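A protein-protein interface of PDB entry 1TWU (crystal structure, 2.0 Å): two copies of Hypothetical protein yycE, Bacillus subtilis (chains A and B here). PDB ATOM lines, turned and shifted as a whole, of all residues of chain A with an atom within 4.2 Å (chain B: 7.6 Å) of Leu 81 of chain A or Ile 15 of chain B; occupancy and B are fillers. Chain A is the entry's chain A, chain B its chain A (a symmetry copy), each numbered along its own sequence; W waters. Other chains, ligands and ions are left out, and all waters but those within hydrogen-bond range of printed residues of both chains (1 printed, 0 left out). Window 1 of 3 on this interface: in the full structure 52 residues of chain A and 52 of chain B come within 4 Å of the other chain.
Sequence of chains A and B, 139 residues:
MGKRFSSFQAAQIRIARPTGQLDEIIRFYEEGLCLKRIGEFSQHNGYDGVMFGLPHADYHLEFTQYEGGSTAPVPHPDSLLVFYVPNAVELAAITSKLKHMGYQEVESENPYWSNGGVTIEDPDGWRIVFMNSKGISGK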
ATOM      1  N   LEU A  80       1.638 -14.320 -31.360  1.00  0.00           N
ATOM      2  CA  LEU A  80       1.018 -13.054 -30.984  1.00  0.00           C
ATOM      3  C   LEU A  80       1.804 -12.097 -30.082  1.00  0.00           C
ATOM      4  O   LEU A  80       2.777 -12.470 -29.418  1.00  0.00           O
ATOM      5  CB  LEU A  80      -0.303 -13.341 -30.257  1.00  0.00           C
ATOM      6  CG  LEU A  80      -1.529 -14.096 -30.794  1.00  0.00           C
ATOM      7  CD1 LEU A  80      -1.290 -14.681 -32.166  1.00  0.00           C
ATOM      8  CD2 LEU A  80      -1.909 -15.170 -29.775  1.00  0.00           C
ATOM      9  N   LEU A  81       1.338 -10.852 -30.081  1.00  0.00           N
ATOM     10  CA  LEU A  81       1.837  -9.789 -29.213  1.00  0.00           C
ATOM     11  C   LEU A  81       0.499  -9.274 -28.690  1.00  0.00           C
ATOM     12  O   LEU A  81      -0.259  -8.647 -29.428  1.00  0.00           O
ATOM     13  CB  LEU A  81       2.562  -8.675 -29.976  1.00  0.00           C
ATOM     14  CG  LEU A  81       2.867  -7.456 -29.083  1.00  0.00           C
ATOM     15  CD1 LEU A  81       3.656  -7.894 -27.860  1.00  0.00           C
ATOM     16  CD2 LEU A  81       3.644  -6.400 -29.853  1.00  0.00           C
ATOM     17  N   VAL A  82       0.195  -9.568 -27.434  1.00  0.00           N
ATOM     18  CA  VAL A  82      -1.079  -9.164 -26.865  1.00  0.00           C
ATOM     19  C   VAL A  82      -1.043  -7.953 -25.936  1.00  0.00           C
ATOM     20  O   VAL A  82      -0.274  -7.903 -24.972  1.00  0.00           O
ATOM     21  CB  VAL A  82      -1.736 -10.333 -26.095  1.00  0.00           C
ATOM     22  CG1 VAL A  82      -3.167  -9.964 -25.722  1.00  0.00           C
ATOM     23  CG2 VAL A  82      -1.712 -11.599 -26.934  1.00  0.00           C
ATOM     24  N   PHE A  83      -1.888  -6.974 -26.244  1.00  0.00           N
ATOM     25  CA  PHE A  83      -2.015  -5.771 -25.437  1.00  0.00           C
ATOM     26  C   PHE A  83      -3.349  -5.889 -24.709  1.00  0.00           C
ATOM     27  O   PHE A  83      -4.395  -5.945 -25.355  1.00  0.00           O
ATOM     28  CB  PHE A  83      -2.047  -4.528 -26.323  1.00  0.00           C
ATOM     29  CG  PHE A  83      -0.702  -4.116 -26.860  1.00  0.00           C
ATOM     30  CD1 PHE A  83       0.260  -3.560 -26.016  1.00  0.00           C
ATOM     31  CD2 PHE A  83      -0.407  -4.254 -28.217  1.00  0.00           C
ATOM     32  CE1 PHE A  83       1.492  -3.144 -26.517  1.00  0.00           C
ATOM     33  CE2 PHE A  83       0.824  -3.843 -28.726  1.00  0.00           C
ATOM     34  CZ  PHE A  83       1.776  -3.285 -27.875  1.00  0.00           C
ATOM     35  N   TRP A 126       2.846 -10.246 -38.145  1.00  0.00           N
ATOM     36  CA  TRP A 126       2.849 -10.577 -36.729  1.00  0.00           C
ATOM     37  C   TRP A 126       1.442 -10.210 -36.263  1.00  0.00           C
ATOM     38  O   TRP A 126       0.915  -9.173 -36.663  1.00  0.00           O
ATOM     39  CB  TRP A 126       3.907  -9.756 -35.981  1.00  0.00           C
ATOM     40  CG  TRP A 126       4.249 -10.316 -34.619  1.00  0.00           C
ATOM     41  CD1 TRP A 126       3.989 -11.585 -34.157  1.00  0.00           C
ATOM     42  CD2 TRP A 126       4.953  -9.646 -33.564  1.00  0.00           C
ATOM     43  NE1 TRP A 126       4.488 -11.738 -32.886  1.00  0.00           N
ATOM     44  CE2 TRP A 126       5.083 -10.566 -32.498  1.00  0.00           C
ATOM     45  CE3 TRP A 126       5.490  -8.359 -33.418  1.00  0.00           C
ATOM     46  CZ2 TRP A 126       5.731 -10.237 -31.301  1.00  0.00           C
ATOM     47  CZ3 TRP A 126       6.136  -8.035 -32.230  1.00  0.00           C
ATOM     48  CH2 TRP A 126       6.249  -8.971 -31.189  1.00  0.00           C
ATOM     49  N   ARG A 127       0.828 -11.069 -35.452  1.00  0.00           N
ATOM     50  CA  ARG A 127      -0.528 -10.833 -34.959  1.00  0.00           C
ATOM     51  C   ARG A 127      -0.543  -9.937 -33.714  1.00  0.00           C
ATOM     52  O   ARG A 127      -0.129 -10.346 -32.628  1.00  0.00           O
ATOM     53  CB  ARG A 127      -1.218 -12.170 -34.635  1.00  0.00           C
ATOM     54  CG  ARG A 127      -1.445 -13.111 -35.828  1.00  0.00           C
ATOM     55  CD  ARG A 127      -2.467 -12.551 -36.795  1.00  0.00           C
ATOM     56  NE  ARG A 127      -2.625 -13.361 -38.005  1.00  0.00           N
ATOM     57  CZ  ARG A 127      -3.518 -14.337 -38.163  1.00  0.00           C
ATOM     58  NH1 ARG A 127      -4.356 -14.659 -37.188  1.00  0.00           N
ATOM     59  NH2 ARG A 127      -3.596 -14.973 -39.321  1.00  0.00           N
ATOM     60  N   ILE A 128      -1.019  -8.709 -33.884  1.00  0.00           N
ATOM     61  CA  ILE A 128      -1.097  -7.769 -32.774  1.00  0.00           C
ATOM     62  C   ILE A 128      -2.531  -7.829 -32.223  1.00  0.00           C
ATOM     63  O   ILE A 128      -3.497  -7.430 -32.884  1.00  0.00           O
ATOM     64  CB  ILE A 128      -0.752  -6.322 -33.233  1.00  0.00           C
ATOM     65  CG1 ILE A 128       0.507  -6.336 -34.108  1.00  0.00           C
ATOM     66  CG2 ILE A 128      -0.516  -5.426 -32.018  1.00  0.00           C
ATOM     67  CD1 ILE A 128       1.707  -6.991 -33.460  1.00  0.00           C
ATOM     68  N   VAL A 129      -2.663  -8.340 -31.006  1.00  0.00           N
ATOM     69  CA  VAL A 129      -3.972  -8.480 -30.390  1.00  0.00           C
ATOM     70  C   VAL A 129      -4.248  -7.449 -29.304  1.00  0.00           C
ATOM     71  O   VAL A 129      -3.383  -7.113 -28.495  1.00  0.00           O
ATOM     72  CB  VAL A 129      -4.141  -9.903 -29.791  1.00  0.00           C
ATOM     73  CG1 VAL A 129      -5.585 -10.128 -29.334  1.00  0.00           C
ATOM     74  CG2 VAL A 129      -3.737 -10.939 -30.823  1.00  0.00           C
ATOM     75  N   ILE B  13       0.984  -7.243 -20.876  1.00  0.00           N
ATOM     76  CA  ILE B  13       1.516  -7.511 -22.207  1.00  0.00           C
ATOM     77  C   ILE B  13       1.958  -8.968 -22.265  1.00  0.00           C
ATOM     78  O   ILE B  13       2.637  -9.465 -21.359  1.00  0.00           O
ATOM     79  CB  ILE B  13       2.710  -6.596 -22.563  1.00  0.00           C
ATOM     80  CG1 ILE B  13       2.246  -5.144 -22.609  1.00  0.00           C
ATOM     81  CG2 ILE B  13       3.276  -6.977 -23.934  1.00  0.00           C
ATOM     82  CD1 ILE B  13       3.332  -4.182 -22.997  1.00  0.00           C
ATOM     83  N   ARG B  14       1.551  -9.644 -23.333  1.00  0.00           N
ATOM     84  CA  ARG B  14       1.869 -11.046 -23.529  1.00  0.00           C
ATOM     85  C   ARG B  14       2.482 -11.337 -24.895  1.00  0.00           C
ATOM     86  O   ARG B  14       2.028 -10.819 -25.918  1.00  0.00           O
ATOM     87  CB  ARG B  14       0.602 -11.896 -23.364  1.00  0.00           C
ATOM     88  CG  ARG B  14       0.786 -13.366 -23.744  1.00  0.00           C
ATOM     89  CD  ARG B  14      -0.509 -14.154 -23.673  1.00  0.00           C
ATOM     90  NE  ARG B  14      -0.977 -14.319 -22.298  1.00  0.00           N
ATOM     91  CZ  ARG B  14      -2.097 -14.949 -21.946  1.00  0.00           C
ATOM     92  NH1 ARG B  14      -2.883 -15.485 -22.869  1.00  0.00           N
ATOM     93  NH2 ARG B  14      -2.433 -15.044 -20.666  1.00  0.00           N
ATOM     94  N   ILE B  15       3.530 -12.157 -24.890  1.00  0.00           N
ATOM     95  CA  ILE B  15       4.188 -12.609 -26.113  1.00  0.00           C
ATOM     96  C   ILE B  15       3.737 -14.062 -26.179  1.00  0.00           C
ATOM     97  O   ILE B  15       4.103 -14.861 -25.311  1.00  0.00           O
ATOM     98  CB  ILE B  15       5.720 -12.594 -25.995  1.00  0.00           C
ATOM     99  CG1 ILE B  15       6.219 -11.162 -25.823  1.00  0.00           C
ATOM    100  CG2 ILE B  15       6.339 -13.210 -27.237  1.00  0.00           C
ATOM    101  CD1 ILE B  15       5.982 -10.285 -27.042  1.00  0.00           C
ATOM    102  N   ALA B  16       2.922 -14.398 -27.176  1.00  0.00           N
ATOM    103  CA  ALA B  16       2.415 -15.763 -27.324  1.00  0.00           C
ATOM    104  C   ALA B  16       3.023 -16.438 -28.541  1.00  0.00           C
ATOM    105  O   ALA B  16       3.021 -15.879 -29.633  1.00  0.00           O
ATOM    106  CB  ALA B  16       0.900 -15.749 -27.436  1.00  0.00           C
ATOM    107  N   ARG B  17       3.547 -17.641 -28.332  1.00  0.00           N
ATOM    108  CA  ARG B  17       4.174 -18.424 -29.392  1.00  0.00           C
ATOM    109  C   ARG B  17       3.644 -19.852 -29.393  1.00  0.00           C
ATOM    110  O   ARG B  17       3.375 -20.428 -28.340  1.00  0.00           O
ATOM    111  CB  ARG B  17       5.695 -18.459 -29.201  1.00  0.00           C
ATOM    112  CG  ARG B  17       6.371 -17.093 -29.266  1.00  0.00           C
ATOM    113  CD  ARG B  17       7.815 -17.161 -28.770  1.00  0.00           C
ATOM    114  NE  ARG B  17       8.619 -18.121 -29.521  1.00  0.00           N
ATOM    115  CZ  ARG B  17       9.131 -17.895 -30.728  1.00  0.00           C
ATOM    116  NH1 ARG B  17       8.929 -16.727 -31.332  1.00  0.00           N
ATOM    117  NH2 ARG B  17       9.841 -18.843 -31.335  1.00  0.00           N
ATOM    118  N   VAL B  50       0.728 -22.705 -21.340  1.00  0.00           N
ATOM    119  CA  VAL B  50       1.344 -22.347 -20.075  1.00  0.00           C
ATOM    120  C   VAL B  50       1.875 -20.922 -20.175  1.00  0.00           C
ATOM    121  O   VAL B  50       2.320 -20.491 -21.234  1.00  0.00           O
ATOM    122  CB  VAL B  50       2.493 -23.336 -19.736  1.00  0.00           C
ATOM    123  CG1 VAL B  50       3.615 -23.212 -20.761  1.00  0.00           C
ATOM    124  CG2 VAL B  50       2.999 -23.088 -18.333  1.00  0.00           C
ATOM    125  N   PHE B  52       4.501 -17.992 -18.497  1.00  0.00           N
ATOM    126  CA  PHE B  52       5.688 -17.771 -17.663  1.00  0.00           C
ATOM    127  C   PHE B  52       5.913 -16.285 -17.409  1.00  0.00           C
ATOM    128  O   PHE B  52       5.891 -15.479 -18.338  1.00  0.00           O
ATOM    129  CB  PHE B  52       6.940 -18.354 -18.332  1.00  0.00           C
ATOM    130  CG  PHE B  52       6.890 -19.834 -18.510  1.00  0.00           C
ATOM    131  CD1 PHE B  52       6.739 -20.673 -17.406  1.00  0.00           C
ATOM    132  CD2 PHE B  52       6.955 -20.397 -19.778  1.00  0.00           C
ATOM    133  CE1 PHE B  52       6.648 -22.054 -17.565  1.00  0.00           C
ATOM    134  CE2 PHE B  52       6.864 -21.779 -19.948  1.00  0.00           C
ATOM    135  CZ  PHE B  52       6.709 -22.607 -18.838  1.00  0.00           C
ATOM    136  N   LEU B  54       7.695 -12.727 -16.661  1.00  0.00           N
ATOM    137  CA  LEU B  54       8.893 -12.138 -17.229  1.00  0.00           C
ATOM    138  C   LEU B  54       9.253 -10.799 -16.575  1.00  0.00           C
ATOM    139  O   LEU B  54       9.347  -9.775 -17.250  1.00  0.00           O
ATOM    140  CB  LEU B  54       8.687 -11.953 -18.730  1.00  0.00           C
ATOM    141  CG  LEU B  54       9.899 -12.102 -19.637  1.00  0.00           C
ATOM    142  CD1 LEU B  54      10.448 -13.523 -19.572  1.00  0.00           C
ATOM    143  CD2 LEU B  54       9.472 -11.748 -21.042  1.00  0.00           C
ATOM    144  N   TYR B  59       4.345  -8.447 -17.764  1.00  0.00           N
ATOM    145  CA  TYR B  59       4.983  -8.839 -19.010  1.00  0.00           C
ATOM    146  C   TYR B  59       5.265 -10.321 -18.855  1.00  0.00           C
ATOM    147  O   TYR B  59       6.041 -10.718 -17.987  1.00  0.00           O
ATOM    148  CB  TYR B  59       6.308  -8.098 -19.220  1.00  0.00           C
ATOM    149  CG  TYR B  59       6.171  -6.606 -19.419  1.00  0.00           C
ATOM    150  CD1 TYR B  59       6.121  -5.735 -18.327  1.00  0.00           C
ATOM    151  CD2 TYR B  59       6.076  -6.062 -20.704  1.00  0.00           C
ATOM    152  CE1 TYR B  59       5.980  -4.361 -18.515  1.00  0.00           C
ATOM    153  CE2 TYR B  59       5.935  -4.693 -20.902  1.00  0.00           C
ATOM    154  CZ  TYR B  59       5.886  -3.848 -19.806  1.00  0.00           C
ATOM    155  OH  TYR B  59       5.730  -2.488 -20.004  1.00  0.00           O
ATOM    156  N   HIS B  60       4.624 -11.143 -19.678  1.00  0.00           N
ATOM    157  CA  HIS B  60       4.846 -12.576 -19.595  1.00  0.00           C
ATOM    158  C   HIS B  60       4.819 -13.252 -20.956  1.00  0.00           C
ATOM    159  O   HIS B  60       4.460 -12.645 -21.972  1.00  0.00           O
ATOM    160  CB  HIS B  60       3.812 -13.239 -18.670  1.00  0.00           C
ATOM    161  CG  HIS B  60       2.397 -13.134 -19.156  1.00  0.00           C
ATOM    162  ND1 HIS B  60       1.568 -12.084 -18.820  1.00  0.00           N
ATOM    163  CD2 HIS B  60       1.673 -13.938 -19.971  1.00  0.00           C
ATOM    164  CE1 HIS B  60       0.396 -12.246 -19.408  1.00  0.00           C
ATOM    165  NE2 HIS B  60       0.433 -13.363 -20.113  1.00  0.00           N
ATOM    166  N   LEU B  61       5.214 -14.521 -20.958  1.00  0.00           N
ATOM    167  CA  LEU B  61       5.244 -15.331 -22.164  1.00  0.00           C
ATOM    168  C   LEU B  61       4.133 -16.362 -22.069  1.00  0.00           C
ATOM    169  O   LEU B  61       3.739 -16.752 -20.968  1.00  0.00           O
ATOM    170  CB  LEU B  61       6.576 -16.085 -22.273  1.00  0.00           C
ATOM    171  CG  LEU B  61       7.908 -15.336 -22.328  1.00  0.00           C
ATOM    172  CD1 LEU B  61       9.063 -16.337 -22.379  1.00  0.00           C
ATOM    173  CD2 LEU B  61       7.930 -14.438 -23.554  1.00  0.00           C
ATOM    174  N   GLU B  62       3.615 -16.781 -23.217  1.00  0.00           N
ATOM    175  CA  GLU B  62       2.616 -17.840 -23.259  1.00  0.00           C
ATOM    176  C   GLU B  62       2.999 -18.791 -24.386  1.00  0.00           C
ATOM    177  O   GLU B  62       3.391 -18.365 -25.470  1.00  0.00           O
ATOM    178  CB  GLU B  62       1.201 -17.321 -23.524  1.00  0.00           C
ATOM    179  CG  GLU B  62       0.229 -18.488 -23.711  1.00  0.00           C
ATOM    180  CD  GLU B  62      -1.155 -18.082 -24.177  1.00  0.00           C
ATOM    181  OE1 GLU B  62      -1.270 -17.109 -24.952  1.00  0.00           O
ATOM    182  OE2 GLU B  62      -2.130 -18.759 -23.783  1.00  0.00           O
ATOM    183  N   PHE B  63       2.910 -20.086 -24.122  1.00  0.00           N
ATOM    184  CA  PHE B  63       3.218 -21.088 -25.137  1.00  0.00           C
ATOM    185  C   PHE B  63       1.996 -21.982 -25.262  1.00  0.00           C
ATOM    186  O   PHE B  63       1.439 -22.441 -24.256  1.00  0.00           O
ATOM    187  CB  PHE B  63       4.451 -21.907 -24.742  1.00  0.00           C
ATOM    188  CG  PHE B  63       5.742 -21.143 -24.861  1.00  0.00           C
ATOM    189  CD1 PHE B  63       6.415 -21.074 -26.081  1.00  0.00           C
ATOM    190  CD2 PHE B  63       6.269 -20.465 -23.763  1.00  0.00           C
ATOM    191  CE1 PHE B  63       7.594 -20.342 -26.207  1.00  0.00           C
ATOM    192  CE2 PHE B  63       7.451 -19.727 -23.875  1.00  0.00           C
ATOM    193  CZ  PHE B  63       8.116 -19.664 -25.098  1.00  0.00           C
ATOM    194  N   LEU B  81      15.187 -12.843 -28.130  1.00  0.00           N
ATOM    195  CA  LEU B  81      14.586 -12.501 -26.844  1.00  0.00           C
ATOM    196  C   LEU B  81      15.864 -12.175 -26.075  1.00  0.00           C
ATOM    197  O   LEU B  81      16.641 -13.069 -25.748  1.00  0.00           O
ATOM    198  CB  LEU B  81      13.866 -13.681 -26.181  1.00  0.00           C
ATOM    199  CG  LEU B  81      13.451 -13.371 -24.728  1.00  0.00           C
ATOM    200  CD1 LEU B  81      12.602 -12.112 -24.689  1.00  0.00           C
ATOM    201  CD2 LEU B  81      12.681 -14.536 -24.125  1.00  0.00           C
ATOM    202  N   TRP B 126      14.191 -20.519 -30.916  1.00  0.00           N
ATOM    203  CA  TRP B 126      14.109 -19.091 -30.650  1.00  0.00           C
ATOM    204  C   TRP B 126      15.465 -18.753 -30.034  1.00  0.00           C
ATOM    205  O   TRP B 126      15.972 -19.516 -29.213  1.00  0.00           O
ATOM    206  CB  TRP B 126      12.970 -18.786 -29.669  1.00  0.00           C
ATOM    207  CG  TRP B 126      12.563 -17.330 -29.657  1.00  0.00           C
ATOM    208  CD1 TRP B 126      12.845 -16.383 -30.613  1.00  0.00           C
ATOM    209  CD2 TRP B 126      11.762 -16.668 -28.667  1.00  0.00           C
ATOM    210  NE1 TRP B 126      12.271 -15.182 -30.275  1.00  0.00           N
ATOM    211  CE2 TRP B 126      11.601 -15.327 -29.088  1.00  0.00           C
ATOM    212  CE3 TRP B 126      11.161 -17.078 -27.468  1.00  0.00           C
ATOM    213  CZ2 TRP B 126      10.862 -14.395 -28.350  1.00  0.00           C
ATOM    214  CZ3 TRP B 126      10.425 -16.153 -26.738  1.00  0.00           C
ATOM    215  CH2 TRP B 126      10.283 -14.828 -27.182  1.00  0.00           C
HETATM  216  O   HOH W   1       4.959 -13.898 -30.653  1.00  0.00           O
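The backbone NH of Leu 80 of chain A sits at hydrogen-bond distance from the backbone carbonyl oxygen of Ala 16 of chain B (2.7 Å). The backbone NH of Val 82 of chain A is in hydrogen-bond range of the backbone carbonyl oxygen of Arg 14 of chain B, at 2.7 Å.
Water W1 lies within hydrogen-bond range of O of Leu 80 of chain A (2.9 Å), O of Ala 16 of chain B (3.0 Å) and NE1 of Trp 126 of chain A (3.1 Å).
Positions printed for both chains: 81 and 126. Of the 7 pairs that touch across the chains among the printed residues, none has its exchanged pair printed and touching as well.
Leu 80 of chain A touches Arg 14 of chain B. Ile 15 of chain B touches Leu 80 of chain A. O of Arg 14 of chain B touches CA of Leu 81 of chain A, 3.5 Å away. Ile 15 of chain B touches Leu 81 of chain A (CD1 to CD1, 3.4 Å). Val 82 of chain A touches Ile 13 of chain B (O to CA, 3.3 Å).
The backbone NH of Leu 81 of chain A is in hydrogen-bond range of the backbone carbonyl oxygen of Arg 127 of chain A, at 3.0 Å. The backbone carbonyl oxygen (O) of Leu 81 of chain A is in hydrogen-bond range of the backbone NH (N) of Val 129 of chain A, 2.9 Å away. O of Ile 13 of chain B lies within hydrogen-bond range of N of His 60 of chain B (3.1 Å). The side-chain carboxylate of Glu 62 of chain B lies within salt-bridge range of the guanidinium group of Arg 14 of chain B (3.1 Å). The backbone carbonyl oxygen of Ile 15 of chain B sits at hydrogen-bond distance from the backbone NH of Glu 62 of chain B (2.9 Å). The backbone NH of Ile 15 of chain B lies within hydrogen-bond range of the backbone carbonyl oxygen of His 60 of chain B (3.1 Å).
Printed residues of chain B within 4 Å of Leu 80 of chain A: Arg 14 (3.9 Å), Ile 15 (3.6 Å) and Ala 16 (2.7 Å). Of chain B, only Arg 14 and Ile 15 come within 4 Å of Leu 81 of chain A. Printed residues of chain A within 4 Å of Ile 13 of chain B: Val 82. Of the printed residues of chain A, Ile 15 of chain B touches Leu 80 (3.6 Å) and Leu 81 (3.4 Å). Printed residues of chain A within 4 Å of Ala 16 of chain B: Leu 80. Leu 81 of chain B touches none of the printed residues of chain A. The nearest residue of chain B that does not touch Leu 81 of chain A is Ile 13 of chain B (4.05 Å). The nearest printed residue of chain A that does not touch Ile 15 of chain B is Trp 126 of chain A (4.3 Å). The nearest printed residue of chain B that does not touch Leu 80 of chain A is Arg 17 of chain B (4.9 Å).
Of the 15 printed residues of chain B, 4 touch a printed residue of chain A. Printed residues of chain B that touch a printed residue of chain A: Ile 13, Arg 14, Ile 15 and Ala 16. Of the 8 printed residues of chain A, 3 touch a printed residue of chain B. Hydrophobic or aromatic side chains of chain A within 4 Å of the printed part of chain B: Leu 80, Leu 81 and Val 82.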
